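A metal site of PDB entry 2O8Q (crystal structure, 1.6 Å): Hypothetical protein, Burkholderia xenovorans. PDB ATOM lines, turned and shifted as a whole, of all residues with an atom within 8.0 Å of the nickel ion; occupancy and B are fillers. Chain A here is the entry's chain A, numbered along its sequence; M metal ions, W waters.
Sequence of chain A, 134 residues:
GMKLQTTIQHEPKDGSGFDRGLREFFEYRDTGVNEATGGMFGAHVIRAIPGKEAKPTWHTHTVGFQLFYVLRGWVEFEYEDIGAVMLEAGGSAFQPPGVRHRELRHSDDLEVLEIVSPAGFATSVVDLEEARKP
A ring nitrogen (ND1) of His 59 sits at hydrogen-bond distance from the backbone carbonyl oxygen (O) of Thr 57 (2.8 Å).
The side-chain amide oxygen of Gln 95 lies close to a ring nitrogen (NE2) of His 101.
ND1 of His 101 sits at hydrogen-bond distance from O of Val 99, 2.9 Å away.
ND1 of His 61 sits at hydrogen-bond distance from OG1 of Thr 123 (2.8 Å).
The nearest printed residue that does not touch the nickel ion is Gln 95 (4.5 Å).
The nickel ion is bound by NE2 of His 61 (2.1 Å), NE2 of His 59 (2.1 Å), water W3 (2.1 Å), NE2 of His 101 (2.1 Å), water W2 (2.1 Å) and water W1 (2.2 Å).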
ATOM      1  N   THR A  57     -16.615  30.360 -11.104  1.00  0.00           N
ATOM      2  CA  THR A  57     -17.510  29.869 -12.125  1.00  0.00           C
ATOM      3  C   THR A  57     -18.954  29.878 -11.601  1.00  0.00           C
ATOM      4  O   THR A  57     -19.189  29.294 -10.554  1.00  0.00           O
ATOM      5  CB  THR A  57     -17.107  28.426 -12.448  1.00  0.00           C
ATOM      6  OG1 THR A  57     -15.713  28.439 -12.809  1.00  0.00           O
ATOM      7  CG2 THR A  57     -17.895  27.921 -13.593  1.00  0.00           C
ATOM      8  N   TRP A  58     -19.842  30.610 -12.287  1.00  0.00           N
ATOM      9  CA  TRP A  58     -21.266  30.588 -11.948  1.00  0.00           C
ATOM     10  C   TRP A  58     -21.779  29.173 -12.017  1.00  0.00           C
ATOM     11  O   TRP A  58     -21.541  28.440 -12.978  1.00  0.00           O
ATOM     12  CB  TRP A  58     -22.060  31.479 -12.888  1.00  0.00           C
ATOM     13  CG  TRP A  58     -21.860  32.936 -12.662  1.00  0.00           C
ATOM     14  CD1 TRP A  58     -21.082  33.787 -13.428  1.00  0.00           C
ATOM     15  CD2 TRP A  58     -22.487  33.787 -11.679  1.00  0.00           C
ATOM     16  NE1 TRP A  58     -21.151  35.069 -12.961  1.00  0.00           N
ATOM     17  CE2 TRP A  58     -22.037  35.110 -11.920  1.00  0.00           C
ATOM     18  CE3 TRP A  58     -23.404  33.571 -10.649  1.00  0.00           C
ATOM     19  CZ2 TRP A  58     -22.431  36.183 -11.138  1.00  0.00           C
ATOM     20  CZ3 TRP A  58     -23.822  34.626  -9.898  1.00  0.00           C
ATOM     21  CH2 TRP A  58     -23.322  35.915 -10.128  1.00  0.00           C
ATOM     22  N   HIS A  59     -22.515  28.752 -10.986  1.00  0.00           N
ATOM     23  CA  HIS A  59     -23.011  27.390 -10.933  1.00  0.00           C
ATOM     24  C   HIS A  59     -24.234  27.334 -10.029  1.00  0.00           C
ATOM     25  O   HIS A  59     -24.587  28.320  -9.365  1.00  0.00           O
ATOM     26  CB  HIS A  59     -21.917  26.415 -10.410  1.00  0.00           C
ATOM     27  CG  HIS A  59     -21.500  26.681  -8.996  1.00  0.00           C
ATOM     28  ND1 HIS A  59     -20.518  27.605  -8.692  1.00  0.00           N
ATOM     29  CD2 HIS A  59     -21.910  26.165  -7.826  1.00  0.00           C
ATOM     30  CE1 HIS A  59     -20.343  27.616  -7.376  1.00  0.00           C
ATOM     31  NE2 HIS A  59     -21.174  26.755  -6.819  1.00  0.00           N
ATOM     32  N   THR A  60     -24.868  26.167 -10.004  1.00  0.00           N
ATOM     33  CA  THR A  60     -25.989  25.854  -9.155  1.00  0.00           C
ATOM     34  C   THR A  60     -25.797  24.459  -8.557  1.00  0.00           C
ATOM     35  O   THR A  60     -25.080  23.631  -9.092  1.00  0.00           O
ATOM     36  CB  THR A  60     -27.328  25.848  -9.935  1.00  0.00           C
ATOM     37  OG1 THR A  60     -27.305  24.775 -10.904  1.00  0.00           O
ATOM     38  CG2 THR A  60     -27.534  27.156 -10.687  1.00  0.00           C
ATOM     39  N   HIS A  61     -26.496  24.235  -7.464  1.00  0.00           N
ATOM     40  CA  HIS A  61     -26.537  22.915  -6.829  1.00  0.00           C
ATOM     41  C   HIS A  61     -27.964  22.412  -6.756  1.00  0.00           C
ATOM     42  O   HIS A  61     -28.874  23.203  -6.494  1.00  0.00           O
ATOM     43  CB  HIS A  61     -25.956  22.960  -5.422  1.00  0.00           C
ATOM     44  CG  HIS A  61     -24.606  23.593  -5.356  1.00  0.00           C
ATOM     45  ND1 HIS A  61     -23.479  23.022  -5.905  1.00  0.00           N
ATOM     46  CD2 HIS A  61     -24.228  24.760  -4.790  1.00  0.00           C
ATOM     47  CE1 HIS A  61     -22.453  23.846  -5.713  1.00  0.00           C
ATOM     48  NE2 HIS A  61     -22.875  24.919  -5.047  1.00  0.00           N
ATOM     49  N   GLN A  66     -29.798  24.692   1.885  1.00  0.00           N
ATOM     50  CA  GLN A  66     -28.375  24.897   1.910  1.00  0.00           C
ATOM     51  C   GLN A  66     -27.984  26.140   2.737  1.00  0.00           C
ATOM     52  O   GLN A  66     -28.418  27.237   2.451  1.00  0.00           O
ATOM     53  CB  GLN A  66     -27.848  25.059   0.474  1.00  0.00           C
ATOM     54  CG  GLN A  66     -26.336  25.144   0.424  1.00  0.00           C
ATOM     55  CD  GLN A  66     -25.816  25.020  -1.015  1.00  0.00           C
ATOM     56  OE1 GLN A  66     -26.346  25.700  -1.916  1.00  0.00           O
ATOM     57  NE2 GLN A  66     -24.788  24.157  -1.216  1.00  0.00           N
ATOM     58  N   PHE A  68     -24.523  28.081   4.839  1.00  0.00           N
ATOM     59  CA  PHE A  68     -23.125  28.184   5.240  1.00  0.00           C
ATOM     60  C   PHE A  68     -23.021  29.079   6.462  1.00  0.00           C
ATOM     61  O   PHE A  68     -23.709  30.115   6.557  1.00  0.00           O
ATOM     62  CB  PHE A  68     -22.298  28.846   4.135  1.00  0.00           C
ATOM     63  CG  PHE A  68     -22.215  27.981   2.908  1.00  0.00           C
ATOM     64  CD1 PHE A  68     -21.281  26.947   2.830  1.00  0.00           C
ATOM     65  CD2 PHE A  68     -23.158  28.072   1.924  1.00  0.00           C
ATOM     66  CE1 PHE A  68     -21.259  26.106   1.735  1.00  0.00           C
ATOM     67  CE2 PHE A  68     -23.118  27.220   0.851  1.00  0.00           C
ATOM     68  CZ  PHE A  68     -22.199  26.247   0.759  1.00  0.00           C
ATOM     69  N   PHE A  77     -18.764  35.561  -1.780  1.00  0.00           N
ATOM     70  CA  PHE A  77     -19.633  34.905  -2.734  1.00  0.00           C
ATOM     71  C   PHE A  77     -20.289  35.960  -3.602  1.00  0.00           C
ATOM     72  O   PHE A  77     -20.259  37.175  -3.319  1.00  0.00           O
ATOM     73  CB  PHE A  77     -20.752  34.190  -1.964  1.00  0.00           C
ATOM     74  CG  PHE A  77     -20.281  33.041  -1.096  1.00  0.00           C
ATOM     75  CD1 PHE A  77     -19.512  32.038  -1.645  1.00  0.00           C
ATOM     76  CD2 PHE A  77     -20.668  32.930   0.232  1.00  0.00           C
ATOM     77  CE1 PHE A  77     -19.089  30.946  -0.863  1.00  0.00           C
ATOM     78  CE2 PHE A  77     -20.298  31.828   1.013  1.00  0.00           C
ATOM     79  CZ  PHE A  77     -19.517  30.849   0.479  1.00  0.00           C
ATOM     80  N   TYR A  79     -24.026  36.336  -5.867  1.00  0.00           N
ATOM     81  CA  TYR A  79     -25.320  35.740  -6.116  1.00  0.00           C
ATOM     82  C   TYR A  79     -26.042  36.435  -7.222  1.00  0.00           C
ATOM     83  O   TYR A  79     -25.926  37.644  -7.375  1.00  0.00           O
ATOM     84  CB  TYR A  79     -26.210  35.792  -4.871  1.00  0.00           C
ATOM     85  CG  TYR A  79     -25.610  34.955  -3.784  1.00  0.00           C
ATOM     86  CD1 TYR A  79     -25.769  33.542  -3.733  1.00  0.00           C
ATOM     87  CD2 TYR A  79     -24.853  35.553  -2.750  1.00  0.00           C
ATOM     88  CE1 TYR A  79     -25.161  32.801  -2.788  1.00  0.00           C
ATOM     89  CE2 TYR A  79     -24.250  34.790  -1.797  1.00  0.00           C
ATOM     90  CZ  TYR A  79     -24.444  33.412  -1.770  1.00  0.00           C
ATOM     91  OH  TYR A  79     -23.839  32.653  -0.830  1.00  0.00           O
ATOM     92  N   GLN A  95     -28.607  29.779   0.948  1.00  0.00           N
ATOM     93  CA  GLN A  95     -28.642  29.740  -0.500  1.00  0.00           C
ATOM     94  C   GLN A  95     -29.903  29.002  -0.927  1.00  0.00           C
ATOM     95  O   GLN A  95     -30.011  27.799  -0.763  1.00  0.00           O
ATOM     96  CB  GLN A  95     -27.441  29.033  -1.064  1.00  0.00           C
ATOM     97  CG  GLN A  95     -26.158  29.747  -0.709  1.00  0.00           C
ATOM     98  CD  GLN A  95     -24.934  29.260  -1.480  1.00  0.00           C
ATOM     99  OE1 GLN A  95     -24.941  28.169  -2.169  1.00  0.00           O
ATOM    100  NE2 GLN A  95     -23.857  30.047  -1.404  1.00  0.00           N
ATOM    101  N   VAL A  99     -29.966  28.324  -6.525  1.00  0.00           N
ATOM    102  CA  VAL A  99     -29.610  29.706  -6.797  1.00  0.00           C
ATOM    103  C   VAL A  99     -28.307  29.759  -7.603  1.00  0.00           C
ATOM    104  O   VAL A  99     -27.382  28.976  -7.320  1.00  0.00           O
ATOM    105  CB  VAL A  99     -29.490  30.563  -5.495  1.00  0.00           C
ATOM    106  CG1 VAL A  99     -28.353  30.179  -4.645  1.00  0.00           C
ATOM    107  CG2 VAL A  99     -29.380  32.066  -5.838  1.00  0.00           C
ATOM    108  N   ARG A 100     -28.253  30.634  -8.625  1.00  0.00           N
ATOM    109  CA  ARG A 100     -27.029  30.807  -9.391  1.00  0.00           C
ATOM    110  C   ARG A 100     -26.067  31.628  -8.577  1.00  0.00           C
ATOM    111  O   ARG A 100     -26.408  32.691  -8.067  1.00  0.00           O
ATOM    112  CB  ARG A 100     -27.296  31.454 -10.750  1.00  0.00           C
ATOM    113  CG  ARG A 100     -28.111  30.611 -11.685  1.00  0.00           C
ATOM    114  CD  ARG A 100     -28.270  31.367 -13.013  1.00  0.00           C
ATOM    115  NE  ARG A 100     -29.175  30.692 -13.918  1.00  0.00           N
ATOM    116  CZ  ARG A 100     -30.513  30.780 -13.878  1.00  0.00           C
ATOM    117  NH1 ARG A 100     -31.128  31.530 -12.952  1.00  0.00           N
ATOM    118  NH2 ARG A 100     -31.235  30.117 -14.763  1.00  0.00           N
ATOM    119  N   HIS A 101     -24.864  31.100  -8.392  1.00  0.00           N
ATOM    120  CA  HIS A 101     -23.881  31.760  -7.519  1.00  0.00           C
ATOM    121  C   HIS A 101     -22.466  31.352  -7.873  1.00  0.00           C
ATOM    122  O   HIS A 101     -22.223  30.449  -8.668  1.00  0.00           O
ATOM    123  CB  HIS A 101     -24.159  31.449  -6.058  1.00  0.00           C
ATOM    124  CG  HIS A 101     -23.936  30.015  -5.726  1.00  0.00           C
ATOM    125  ND1 HIS A 101     -24.774  29.009  -6.162  1.00  0.00           N
ATOM    126  CD2 HIS A 101     -22.916  29.385  -5.075  1.00  0.00           C
ATOM    127  CE1 HIS A 101     -24.281  27.843  -5.793  1.00  0.00           C
ATOM    128  NE2 HIS A 101     -23.164  28.038  -5.112  1.00  0.00           N
ATOM    129  N   ARG A 102     -21.503  32.029  -7.279  1.00  0.00           N
ATOM    130  CA  ARG A 102     -20.116  31.646  -7.459  1.00  0.00           C
ATOM    131  C   ARG A 102     -19.335  32.141  -6.244  1.00  0.00           C
ATOM    132  O   ARG A 102     -19.845  32.991  -5.498  1.00  0.00           O
ATOM    133  CB  ARG A 102     -19.556  32.174  -8.792  1.00  0.00           C
ATOM    134  CG  ARG A 102     -19.545  33.682  -8.924  1.00  0.00           C
ATOM    135  CD  ARG A 102     -18.914  34.143 -10.223  1.00  0.00           C
ATOM    136  NE  ARG A 102     -18.965  35.578 -10.421  1.00  0.00           N
ATOM    137  CZ  ARG A 102     -18.326  36.206 -11.411  1.00  0.00           C
ATOM    138  NH1 ARG A 102     -17.585  35.493 -12.258  1.00  0.00           N
ATOM    139  NH2 ARG A 102     -18.419  37.526 -11.558  1.00  0.00           N
ATOM    140  N   GLU A 103     -18.149  31.571  -6.051  1.00  0.00           N
ATOM    141  CA  GLU A 103     -17.238  32.013  -4.983  1.00  0.00           C
ATOM    142  C   GLU A 103     -16.136  32.828  -5.623  1.00  0.00           C
ATOM    143  O   GLU A 103     -15.485  32.358  -6.544  1.00  0.00           O
ATOM    144  CB  GLU A 103     -16.594  30.854  -4.252  1.00  0.00           C
ATOM    145  CG  GLU A 103     -15.814  31.313  -3.025  1.00  0.00           C
ATOM    146  CD  GLU A 103     -14.357  30.861  -3.060  1.00  0.00           C
ATOM    147  OE1 GLU A 103     -14.063  29.742  -3.570  1.00  0.00           O
ATOM    148  OE2 GLU A 103     -13.510  31.640  -2.585  1.00  0.00           O
ATOM    149  N   GLU A 114     -21.062  23.810   6.278  1.00  0.00           N
ATOM    150  CA  GLU A 114     -22.102  23.704   5.270  1.00  0.00           C
ATOM    151  C   GLU A 114     -23.098  22.658   5.766  1.00  0.00           C
ATOM    152  O   GLU A 114     -22.683  21.569   6.141  1.00  0.00           O
ATOM    153  CB  GLU A 114     -21.576  23.251   3.892  1.00  0.00           C
ATOM    154  CG  GLU A 114     -22.666  23.125   2.804  1.00  0.00           C
ATOM    155  CD  GLU A 114     -22.132  22.782   1.445  1.00  0.00           C
ATOM    156  OE1 GLU A 114     -20.991  22.244   1.329  1.00  0.00           O
ATOM    157  OE2 GLU A 114     -22.844  23.033   0.426  1.00  0.00           O
ATOM    158  N   PHE A 121     -25.984  16.073  -3.547  1.00  0.00           N
ATOM    159  CA  PHE A 121     -26.432  16.992  -4.613  1.00  0.00           C
ATOM    160  C   PHE A 121     -25.504  17.022  -5.836  1.00  0.00           C
ATOM    161  O   PHE A 121     -24.260  16.759  -5.769  1.00  0.00           O
ATOM    162  CB  PHE A 121     -26.645  18.376  -4.045  1.00  0.00           C
ATOM    163  CG  PHE A 121     -25.416  18.986  -3.429  1.00  0.00           C
ATOM    164  CD1 PHE A 121     -25.063  18.774  -2.118  1.00  0.00           C
ATOM    165  CD2 PHE A 121     -24.572  19.767  -4.215  1.00  0.00           C
ATOM    166  CE1 PHE A 121     -23.920  19.329  -1.581  1.00  0.00           C
ATOM    167  CE2 PHE A 121     -23.444  20.316  -3.682  1.00  0.00           C
ATOM    168  CZ  PHE A 121     -23.116  20.098  -2.339  1.00  0.00           C
ATOM    169  N   THR A 123     -23.925  19.388  -9.117  1.00  0.00           N
ATOM    170  CA  THR A 123     -23.518  20.777  -9.374  1.00  0.00           C
ATOM    171  C   THR A 123     -23.441  20.977 -10.871  1.00  0.00           C
ATOM    172  O   THR A 123     -22.902  20.141 -11.579  1.00  0.00           O
ATOM    173  CB  THR A 123     -22.152  21.023  -8.698  1.00  0.00           C
ATOM    174  OG1 THR A 123     -22.276  20.885  -7.270  1.00  0.00           O
ATOM    175  CG2 THR A 123     -21.633  22.438  -9.037  1.00  0.00           C
HETATM  176 NI    NI M   1     -21.638  26.568  -4.796  1.00  0.00          NI
HETATM  177  O   HOH W   1     -20.254  28.137  -4.275  1.00  0.00           O
HETATM  178  O   HOH W   2     -19.931  25.292  -4.527  1.00  0.00           O
HETATM  179  O   HOH W   3     -22.122  26.435  -2.730  1.00  0.00           O
